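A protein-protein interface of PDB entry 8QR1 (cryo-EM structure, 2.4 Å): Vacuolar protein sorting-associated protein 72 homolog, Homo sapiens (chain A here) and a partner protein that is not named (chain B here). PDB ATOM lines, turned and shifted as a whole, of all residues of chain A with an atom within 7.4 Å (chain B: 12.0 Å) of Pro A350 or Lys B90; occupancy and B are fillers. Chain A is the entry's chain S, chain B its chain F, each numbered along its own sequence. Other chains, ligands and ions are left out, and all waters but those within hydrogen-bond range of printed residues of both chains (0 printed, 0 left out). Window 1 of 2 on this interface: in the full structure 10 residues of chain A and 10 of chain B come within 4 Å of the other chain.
The side-chain amino group of Lys B90 sits close to a ring nitrogen (NE2) of His A296. N of Lys B91 sits at hydrogen-bond distance from O of Pro A348 (2.6 Å). The backbone carbonyl oxygen (O) of Pro A346 lies close to the guanidinium group (NH1) of Arg B93, at 3.3 Å.
OG of Ser B89 lies within hydrogen-bond range of O of Ala B85. The side-chain hydroxyl of Ser B89 is in hydrogen-bond range of the backbone carbonyl oxygen of Lys B86 (3.1 Å).
Among the printed residues, pairs that only touch across the chains: Glu A347 with Lys B91, Pro A348 with Lys B90, Pro A348 with Arg B93, Pro A350 with Ser B89, Glu A347 with Lys B90, Pro A350 with Lys B90, Leu A349 with Lys B90 and Pro A350 with Gly B88.
No residue of chain B comes within 4 Å of Ala A336. Pro A341 touches none of the printed residues of chain B. Of chain B, only Lys B90 and Lys B91 come within 4 Å of Glu A347. Of the printed residues of chain B, Pro A348 touches Lys B90, Lys B91 and Arg B93. Leu A349 touches just one residue of chain B: Lys B90. No residue of chain B comes within 4 Å of Gly A351. No residue of chain B comes within 4 Å of Ser A352. Of the printed residues of chain A, Arg B93 touches Pro A346 and Pro A348. Of the printed residues of chain A, Ser B89 touches Pro A350 (3.5 Å). Of the printed residues of chain B, His A296 touches Lys B90. Of the printed residues of chain A, Gly B88 touches Pro A350 (3.8 Å). Of the printed residues of chain A, Lys B91 touches Glu A347 and Pro A348. The nearest printed residue of chain B that does not touch His A296 is Ser B89 (4.02 Å).
Of the 14 printed residues of chain B, 5 touch a printed residue of chain A. Printed residues of chain B that touch a printed residue of chain A: Gly B88, Ser B89, Lys B90, Lys B91 and Arg B93. Among the printed residues, no Asp or Glu carboxylate lies within 4 Å of a Lys or Arg side-chain nitrogen of the other chain.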
ATOM      1  N   VAL A 291      13.745 -10.490  18.371  1.00  0.00           N
ATOM      2  CA  VAL A 291      14.573  -9.592  19.165  1.00  0.00           C
ATOM      3  C   VAL A 291      13.651  -8.651  19.923  1.00  0.00           C
ATOM      4  O   VAL A 291      12.650  -8.175  19.377  1.00  0.00           O
ATOM      5  CB  VAL A 291      15.555  -8.793  18.282  1.00  0.00           C
ATOM      6  CG1 VAL A 291      16.337  -7.791  19.131  1.00  0.00           C
ATOM      7  CG2 VAL A 291      16.489  -9.744  17.532  1.00  0.00           C
ATOM      8  N   PRO A 293      12.183  -5.304  21.361  1.00  0.00           N
ATOM      9  CA  PRO A 293      12.340  -3.888  20.990  1.00  0.00           C
ATOM     10  C   PRO A 293      13.114  -3.064  22.005  1.00  0.00           C
ATOM     11  O   PRO A 293      13.666  -2.022  21.630  1.00  0.00           O
ATOM     12  CB  PRO A 293      10.893  -3.393  20.864  1.00  0.00           C
ATOM     13  CG  PRO A 293      10.102  -4.598  20.610  1.00  0.00           C
ATOM     14  CD  PRO A 293      10.753  -5.667  21.410  1.00  0.00           C
ATOM     15  N   HIS A 296      17.145  -4.910  23.104  1.00  0.00           N
ATOM     16  CA  HIS A 296      17.521  -5.991  22.198  1.00  0.00           C
ATOM     17  C   HIS A 296      17.790  -7.296  22.959  1.00  0.00           C
ATOM     18  O   HIS A 296      17.103  -7.563  23.948  1.00  0.00           O
ATOM     19  CB  HIS A 296      18.702  -5.524  21.338  1.00  0.00           C
ATOM     20  CG  HIS A 296      18.435  -4.249  20.602  1.00  0.00           C
ATOM     21  ND1 HIS A 296      17.189  -3.926  20.110  1.00  0.00           N
ATOM     22  CD2 HIS A 296      19.253  -3.227  20.258  1.00  0.00           C
ATOM     23  CE1 HIS A 296      17.248  -2.753  19.505  1.00  0.00           C
ATOM     24  NE2 HIS A 296      18.489  -2.309  19.578  1.00  0.00           N
ATOM     25  N   ARG A 297      18.764  -8.130  22.503  1.00  0.00           N
ATOM     26  CA  ARG A 297      19.011  -9.516  22.908  1.00  0.00           C
ATOM     27  C   ARG A 297      17.872 -10.417  22.429  1.00  0.00           C
ATOM     28  O   ARG A 297      16.812  -9.911  22.040  1.00  0.00           O
ATOM     29  CB  ARG A 297      19.219  -9.652  24.425  1.00  0.00           C
ATOM     30  CG  ARG A 297      20.414  -8.868  24.952  1.00  0.00           C
ATOM     31  CD  ARG A 297      20.949  -9.435  26.264  1.00  0.00           C
ATOM     32  NE  ARG A 297      20.001  -9.289  27.366  1.00  0.00           N
ATOM     33  CZ  ARG A 297      19.865  -8.214  28.136  1.00  0.00           C
ATOM     34  NH1 ARG A 297      20.586  -7.116  27.947  1.00  0.00           N
ATOM     35  NH2 ARG A 297      18.978  -8.238  29.126  1.00  0.00           N
ATOM     36  N   THR A 335       6.187   5.356  19.978  1.00  0.00           N
ATOM     37  CA  THR A 335       7.397   4.562  20.183  1.00  0.00           C
ATOM     38  C   THR A 335       8.696   5.248  19.783  1.00  0.00           C
ATOM     39  O   THR A 335       9.747   4.601  19.854  1.00  0.00           O
ATOM     40  CB  THR A 335       7.296   3.246  19.401  1.00  0.00           C
ATOM     41  N   ALA A 336       8.673   6.512  19.374  1.00  0.00           N
ATOM     42  CA  ALA A 336       9.891   7.189  18.934  1.00  0.00           C
ATOM     43  C   ALA A 336      10.766   7.474  20.147  1.00  0.00           C
ATOM     44  O   ALA A 336      10.614   8.503  20.809  1.00  0.00           O
ATOM     45  CB  ALA A 336       9.544   8.473  18.191  1.00  0.00           C
ATOM     46  N   SER A 337      11.705   6.564  20.429  1.00  0.00           N
ATOM     47  CA  SER A 337      12.587   6.671  21.593  1.00  0.00           C
ATOM     48  C   SER A 337      11.785   6.734  22.890  1.00  0.00           C
ATOM     49  O   SER A 337      12.079   7.530  23.784  1.00  0.00           O
ATOM     50  CB  SER A 337      13.509   7.886  21.473  1.00  0.00           C
ATOM     51  N   ALA A 338      10.765   5.888  22.995  1.00  0.00           N
ATOM     52  CA  ALA A 338       9.825   5.978  24.103  1.00  0.00           C
ATOM     53  C   ALA A 338      10.407   5.355  25.367  1.00  0.00           C
ATOM     54  O   ALA A 338      10.750   4.169  25.390  1.00  0.00           O
ATOM     55  CB  ALA A 338       8.514   5.289  23.730  1.00  0.00           C
ATOM     56  N   PRO A 341      14.275   3.336  25.301  1.00  0.00           N
ATOM     57  CA  PRO A 341      14.233   1.910  24.963  1.00  0.00           C
ATOM     58  C   PRO A 341      15.579   1.386  24.479  1.00  0.00           C
ATOM     59  O   PRO A 341      15.717   0.961  23.327  1.00  0.00           O
ATOM     60  CB  PRO A 341      13.161   1.870  23.869  1.00  0.00           C
ATOM     61  CG  PRO A 341      13.409   3.137  23.121  1.00  0.00           C
ATOM     62  CD  PRO A 341      13.817   4.162  24.168  1.00  0.00           C
ATOM     63  N   GLY A 342      16.584   1.418  25.351  1.00  0.00           N
ATOM     64  CA  GLY A 342      17.897   0.932  24.997  1.00  0.00           C
ATOM     65  C   GLY A 342      18.539   1.792  23.926  1.00  0.00           C
ATOM     66  O   GLY A 342      18.696   1.355  22.782  1.00  0.00           O
ATOM     67  N   PRO A 344      21.724   3.290  23.265  1.00  0.00           N
ATOM     68  CA  PRO A 344      23.097   3.567  22.797  1.00  0.00           C
ATOM     69  C   PRO A 344      23.243   3.137  21.345  1.00  0.00           C
ATOM     70  O   PRO A 344      22.923   1.981  21.035  1.00  0.00           O
ATOM     71  CB  PRO A 344      23.976   2.718  23.724  1.00  0.00           C
ATOM     72  CG  PRO A 344      23.187   1.588  24.021  1.00  0.00           C
ATOM     73  CD  PRO A 344      21.754   2.018  24.026  1.00  0.00           C
ATOM     74  N   PRO A 345      23.575   4.045  20.413  1.00  0.00           N
ATOM     75  CA  PRO A 345      23.648   3.670  18.987  1.00  0.00           C
ATOM     76  C   PRO A 345      25.055   3.339  18.510  1.00  0.00           C
ATOM     77  O   PRO A 345      25.735   4.219  17.962  1.00  0.00           O
ATOM     78  CB  PRO A 345      23.107   4.925  18.294  1.00  0.00           C
ATOM     79  CG  PRO A 345      23.653   6.032  19.122  1.00  0.00           C
ATOM     80  CD  PRO A 345      23.841   5.496  20.539  1.00  0.00           C
ATOM     81  N   PRO A 346      25.560   2.111  18.687  1.00  0.00           N
ATOM     82  CA  PRO A 346      26.608   1.668  17.752  1.00  0.00           C
ATOM     83  C   PRO A 346      26.133   1.684  16.312  1.00  0.00           C
ATOM     84  O   PRO A 346      26.906   2.011  15.402  1.00  0.00           O
ATOM     85  CB  PRO A 346      26.938   0.250  18.229  1.00  0.00           C
ATOM     86  CG  PRO A 346      26.618   0.258  19.656  1.00  0.00           C
ATOM     87  CD  PRO A 346      25.443   1.175  19.818  1.00  0.00           C
ATOM     88  N   GLU A 347      24.872   1.327  16.089  1.00  0.00           N
ATOM     89  CA  GLU A 347      24.158   1.468  14.830  1.00  0.00           C
ATOM     90  C   GLU A 347      22.774   1.994  15.221  1.00  0.00           C
ATOM     91  O   GLU A 347      22.094   1.314  15.998  1.00  0.00           O
ATOM     92  CB  GLU A 347      24.094   0.127  14.098  1.00  0.00           C
ATOM     93  CG  GLU A 347      23.386   0.137  12.758  1.00  0.00           C
ATOM     94  CD  GLU A 347      23.291  -1.244  12.136  1.00  0.00           C
ATOM     95  OE1 GLU A 347      23.822  -2.203  12.730  1.00  0.00           O
ATOM     96  OE2 GLU A 347      22.679  -1.371  11.056  1.00  0.00           O
ATOM     97  N   PRO A 348      22.316   3.211  14.755  1.00  0.00           N
ATOM     98  CA  PRO A 348      21.092   3.807  15.324  1.00  0.00           C
ATOM     99  C   PRO A 348      19.824   2.967  15.248  1.00  0.00           C
ATOM    100  O   PRO A 348      19.682   2.098  14.382  1.00  0.00           O
ATOM    101  CB  PRO A 348      20.930   5.094  14.509  1.00  0.00           C
ATOM    102  CG  PRO A 348      22.281   5.478  14.154  1.00  0.00           C
ATOM    103  CD  PRO A 348      23.026   4.204  13.921  1.00  0.00           C
ATOM    104  N   LEU A 349      18.898   3.238  16.175  1.00  0.00           N
ATOM    105  CA  LEU A 349      17.737   2.409  16.454  1.00  0.00           C
ATOM    106  C   LEU A 349      16.473   3.109  15.970  1.00  0.00           C
ATOM    107  O   LEU A 349      16.358   4.326  16.173  1.00  0.00           O
ATOM    108  CB  LEU A 349      17.622   2.150  17.961  1.00  0.00           C
ATOM    109  CG  LEU A 349      18.790   1.555  18.765  1.00  0.00           C
ATOM    110  CD1 LEU A 349      19.490   0.438  18.022  1.00  0.00           C
ATOM    111  CD2 LEU A 349      19.800   2.620  19.194  1.00  0.00           C
ATOM    112  N   PRO A 350      15.507   2.425  15.344  1.00  0.00           N
ATOM    113  CA  PRO A 350      14.190   3.046  15.152  1.00  0.00           C
ATOM    114  C   PRO A 350      13.348   2.966  16.416  1.00  0.00           C
ATOM    115  O   PRO A 350      13.745   2.403  17.438  1.00  0.00           O
ATOM    116  CB  PRO A 350      13.561   2.231  14.017  1.00  0.00           C
ATOM    117  CG  PRO A 350      14.667   1.461  13.422  1.00  0.00           C
ATOM    118  CD  PRO A 350      15.612   1.200  14.536  1.00  0.00           C
ATOM    119  N   GLY A 351      12.153   3.544  16.331  1.00  0.00           N
ATOM    120  CA  GLY A 351      11.226   3.470  17.443  1.00  0.00           C
ATOM    121  C   GLY A 351      10.724   2.055  17.663  1.00  0.00           C
ATOM    122  O   GLY A 351      10.706   1.227  16.751  1.00  0.00           O
ATOM    123  N   SER A 352      10.303   1.785  18.898  1.00  0.00           N
ATOM    124  CA  SER A 352       9.891   0.445  19.300  1.00  0.00           C
ATOM    125  C   SER A 352       8.415   0.202  19.013  1.00  0.00           C
ATOM    126  O   SER A 352       7.659  -0.153  19.925  1.00  0.00           O
ATOM    127  CB  SER A 352      10.171   0.230  20.790  1.00  0.00           C
ATOM    128  OG  SER A 352       9.357   1.068  21.591  1.00  0.00           O
ATOM    129  N   GLY A 353       8.005   0.390  17.755  1.00  0.00           N
ATOM    130  CA  GLY A 353       6.632   0.206  17.330  1.00  0.00           C
ATOM    131  C   GLY A 353       6.409  -0.856  16.264  1.00  0.00           C
ATOM    132  O   GLY A 353       5.657  -0.623  15.312  1.00  0.00           O
ATOM    133  N   ASP B  75      24.848 -12.114   5.589  1.00  0.00           N
ATOM    134  CA  ASP B  75      23.855 -12.150   6.651  1.00  0.00           C
ATOM    135  C   ASP B  75      22.573 -12.855   6.232  1.00  0.00           C
ATOM    136  O   ASP B  75      21.884 -13.425   7.086  1.00  0.00           O
ATOM    137  CB  ASP B  75      23.523 -10.725   7.093  1.00  0.00           C
ATOM    138  CG  ASP B  75      24.712 -10.007   7.684  1.00  0.00           C
ATOM    139  OD1 ASP B  75      25.404 -10.601   8.535  1.00  0.00           O
ATOM    140  OD2 ASP B  75      24.960  -8.848   7.297  1.00  0.00           O
ATOM    141  N   TYR B  80      15.795 -13.944   4.108  1.00  0.00           N
ATOM    142  CA  TYR B  80      15.538 -12.643   4.715  1.00  0.00           C
ATOM    143  C   TYR B  80      14.567 -12.750   5.884  1.00  0.00           C
ATOM    144  O   TYR B  80      14.713 -12.035   6.883  1.00  0.00           O
ATOM    145  CB  TYR B  80      14.993 -11.673   3.670  1.00  0.00           C
ATOM    146  CG  TYR B  80      14.330 -10.457   4.271  1.00  0.00           C
ATOM    147  CD1 TYR B  80      15.064  -9.518   4.974  1.00  0.00           C
ATOM    148  CD2 TYR B  80      12.965 -10.258   4.150  1.00  0.00           C
ATOM    149  CE1 TYR B  80      14.460  -8.411   5.529  1.00  0.00           C
ATOM    150  CE2 TYR B  80      12.354  -9.155   4.703  1.00  0.00           C
ATOM    151  CZ  TYR B  80      13.105  -8.235   5.390  1.00  0.00           C
ATOM    152  OH  TYR B  80      12.495  -7.136   5.945  1.00  0.00           O
ATOM    153  N   VAL B  83      15.955 -13.194   9.371  1.00  0.00           N
ATOM    154  CA  VAL B  83      16.628 -12.056   9.984  1.00  0.00           C
ATOM    155  C   VAL B  83      15.891 -10.746   9.731  1.00  0.00           C
ATOM    156  O   VAL B  83      16.515  -9.687   9.719  1.00  0.00           O
ATOM    157  CB  VAL B  83      18.089 -11.950   9.502  1.00  0.00           C
ATOM    158  CG1 VAL B  83      18.850 -13.218   9.826  1.00  0.00           C
ATOM    159  CG2 VAL B  83      18.178 -11.637   8.008  1.00  0.00           C
ATOM    160  N   LYS B  84      14.573 -10.791   9.528  1.00  0.00           N
ATOM    161  CA  LYS B  84      13.850  -9.561   9.221  1.00  0.00           C
ATOM    162  C   LYS B  84      13.788  -8.638  10.433  1.00  0.00           C
ATOM    163  O   LYS B  84      13.900  -7.416  10.294  1.00  0.00           O
ATOM    164  CB  LYS B  84      12.449  -9.886   8.681  1.00  0.00           C
ATOM    165  CG  LYS B  84      11.420 -10.488   9.650  1.00  0.00           C
ATOM    166  CD  LYS B  84      10.014 -10.435   9.052  1.00  0.00           C
ATOM    167  CE  LYS B  84       8.938 -10.810  10.063  1.00  0.00           C
ATOM    168  NZ  LYS B  84       7.575 -10.431   9.593  1.00  0.00           N
ATOM    169  N   ALA B  85      13.629  -9.203  11.630  1.00  0.00           N
ATOM    170  CA  ALA B  85      13.531  -8.379  12.829  1.00  0.00           C
ATOM    171  C   ALA B  85      14.874  -7.772  13.205  1.00  0.00           C
ATOM    172  O   ALA B  85      14.931  -6.612  13.634  1.00  0.00           O
ATOM    173  CB  ALA B  85      12.986  -9.209  13.987  1.00  0.00           C
ATOM    174  N   LYS B  86      15.955  -8.539  13.052  1.00  0.00           N
ATOM    175  CA  LYS B  86      17.286  -8.054  13.394  1.00  0.00           C
ATOM    176  C   LYS B  86      17.674  -6.859  12.533  1.00  0.00           C
ATOM    177  O   LYS B  86      18.241  -5.880  13.030  1.00  0.00           O
ATOM    178  CB  LYS B  86      18.300  -9.194  13.230  1.00  0.00           C
ATOM    179  CG  LYS B  86      19.687  -9.083  13.912  1.00  0.00           C
ATOM    180  CD  LYS B  86      19.738  -8.423  15.295  1.00  0.00           C
ATOM    181  CE  LYS B  86      21.175  -8.223  15.764  1.00  0.00           C
ATOM    182  NZ  LYS B  86      21.265  -7.265  16.898  1.00  0.00           N
ATOM    183  N   LEU B  87      17.371  -6.923  11.238  1.00  0.00           N
ATOM    184  CA  LEU B  87      17.654  -5.803  10.349  1.00  0.00           C
ATOM    185  C   LEU B  87      16.664  -4.663  10.557  1.00  0.00           C
ATOM    186  O   LEU B  87      17.049  -3.490  10.524  1.00  0.00           O
ATOM    187  CB  LEU B  87      17.626  -6.271   8.896  1.00  0.00           C
ATOM    188  CG  LEU B  87      18.606  -7.377   8.504  1.00  0.00           C
ATOM    189  CD1 LEU B  87      18.284  -7.898   7.122  1.00  0.00           C
ATOM    190  CD2 LEU B  87      20.036  -6.890   8.568  1.00  0.00           C
ATOM    191  N   GLY B  88      15.389  -4.989  10.775  1.00  0.00           N
ATOM    192  CA  GLY B  88      14.371  -3.969  10.936  1.00  0.00           C
ATOM    193  C   GLY B  88      14.475  -3.181  12.223  1.00  0.00           C
ATOM    194  O   GLY B  88      13.929  -2.074  12.299  1.00  0.00           O
ATOM    195  N   SER B  89      15.158  -3.717  13.231  1.00  0.00           N
ATOM    196  CA  SER B  89      15.343  -3.032  14.503  1.00  0.00           C
ATOM    197  C   SER B  89      16.576  -2.133  14.523  1.00  0.00           C
ATOM    198  O   SER B  89      17.036  -1.766  15.609  1.00  0.00           O
ATOM    199  CB  SER B  89      15.443  -4.056  15.635  1.00  0.00           C
ATOM    200  OG  SER B  89      16.559  -4.909  15.455  1.00  0.00           O
ATOM    201  N   LYS B  90      17.114  -1.766  13.359  1.00  0.00           N
ATOM    202  CA  LYS B  90      18.341  -0.993  13.258  1.00  0.00           C
ATOM    203  C   LYS B  90      18.234  -0.018  12.095  1.00  0.00           C
ATOM    204  O   LYS B  90      17.419  -0.187  11.185  1.00  0.00           O
ATOM    205  CB  LYS B  90      19.561  -1.900  13.062  1.00  0.00           C
ATOM    206  CG  LYS B  90      19.986  -2.688  14.293  1.00  0.00           C
ATOM    207  CD  LYS B  90      20.562  -1.801  15.380  1.00  0.00           C
ATOM    208  CE  LYS B  90      21.364  -2.594  16.395  1.00  0.00           C
ATOM    209  NZ  LYS B  90      20.520  -3.535  17.172  1.00  0.00           N
ATOM    210  N   LYS B  91      19.076   1.010  12.149  1.00  0.00           N
ATOM    211  CA  LYS B  91      19.120   2.076  11.157  1.00  0.00           C
ATOM    212  C   LYS B  91      20.578   2.371  10.846  1.00  0.00           C
ATOM    213  O   LYS B  91      21.403   2.448  11.759  1.00  0.00           O
ATOM    214  CB  LYS B  91      18.397   3.317  11.685  1.00  0.00           C
ATOM    215  CG  LYS B  91      18.304   4.493  10.727  1.00  0.00           C
ATOM    216  CD  LYS B  91      17.699   5.723  11.392  1.00  0.00           C
ATOM    217  CE  LYS B  91      16.187   5.638  11.498  1.00  0.00           C
ATOM    218  NZ  LYS B  91      15.525   5.861  10.188  1.00  0.00           N
ATOM    219  N   VAL B  92      20.894   2.539   9.562  1.00  0.00           N
ATOM    220  CA  VAL B  92      22.283   2.712   9.153  1.00  0.00           C
ATOM    221  C   VAL B  92      22.801   4.071   9.593  1.00  0.00           C
ATOM    222  O   VAL B  92      22.058   5.059   9.669  1.00  0.00           O
ATOM    223  CB  VAL B  92      22.459   2.551   7.631  1.00  0.00           C
ATOM    224  CG1 VAL B  92      22.007   1.204   7.182  1.00  0.00           C
ATOM    225  CG2 VAL B  92      21.749   3.658   6.866  1.00  0.00           C
ATOM    226  N   ARG B  93      24.099   4.121   9.874  1.00  0.00           N
ATOM    227  CA  ARG B  93      24.771   5.392  10.063  1.00  0.00           C
ATOM    228  C   ARG B  93      25.009   6.042   8.699  1.00  0.00           C
ATOM    229  O   ARG B  93      25.393   5.353   7.750  1.00  0.00           O
ATOM    230  CB  ARG B  93      26.100   5.191  10.779  1.00  0.00           C
ATOM    231  CG  ARG B  93      25.962   4.809  12.229  1.00  0.00           C
ATOM    232  CD  ARG B  93      27.284   4.401  12.818  1.00  0.00           C
ATOM    233  NE  ARG B  93      27.693   3.081  12.357  1.00  0.00           N
ATOM    234  CZ  ARG B  93      28.772   2.427  12.765  1.00  0.00           C
ATOM    235  NH1 ARG B  93      29.588   2.922  13.683  1.00  0.00           N
ATOM    236  NH2 ARG B  93      29.043   1.237  12.238  1.00  0.00           N
ATOM    237  N   PRO B  94      24.795   7.352   8.555  1.00  0.00           N
ATOM    238  CA  PRO B  94      24.926   7.951   7.223  1.00  0.00           C
ATOM    239  C   PRO B  94      26.381   8.055   6.787  1.00  0.00           C
ATOM    240  O   PRO B  94      27.275   8.282   7.603  1.00  0.00           O
ATOM    241  CB  PRO B  94      24.288   9.329   7.393  1.00  0.00           C
ATOM    242  CG  PRO B  94      24.516   9.657   8.782  1.00  0.00           C
ATOM    243  CD  PRO B  94      24.451   8.383   9.550  1.00  0.00           C
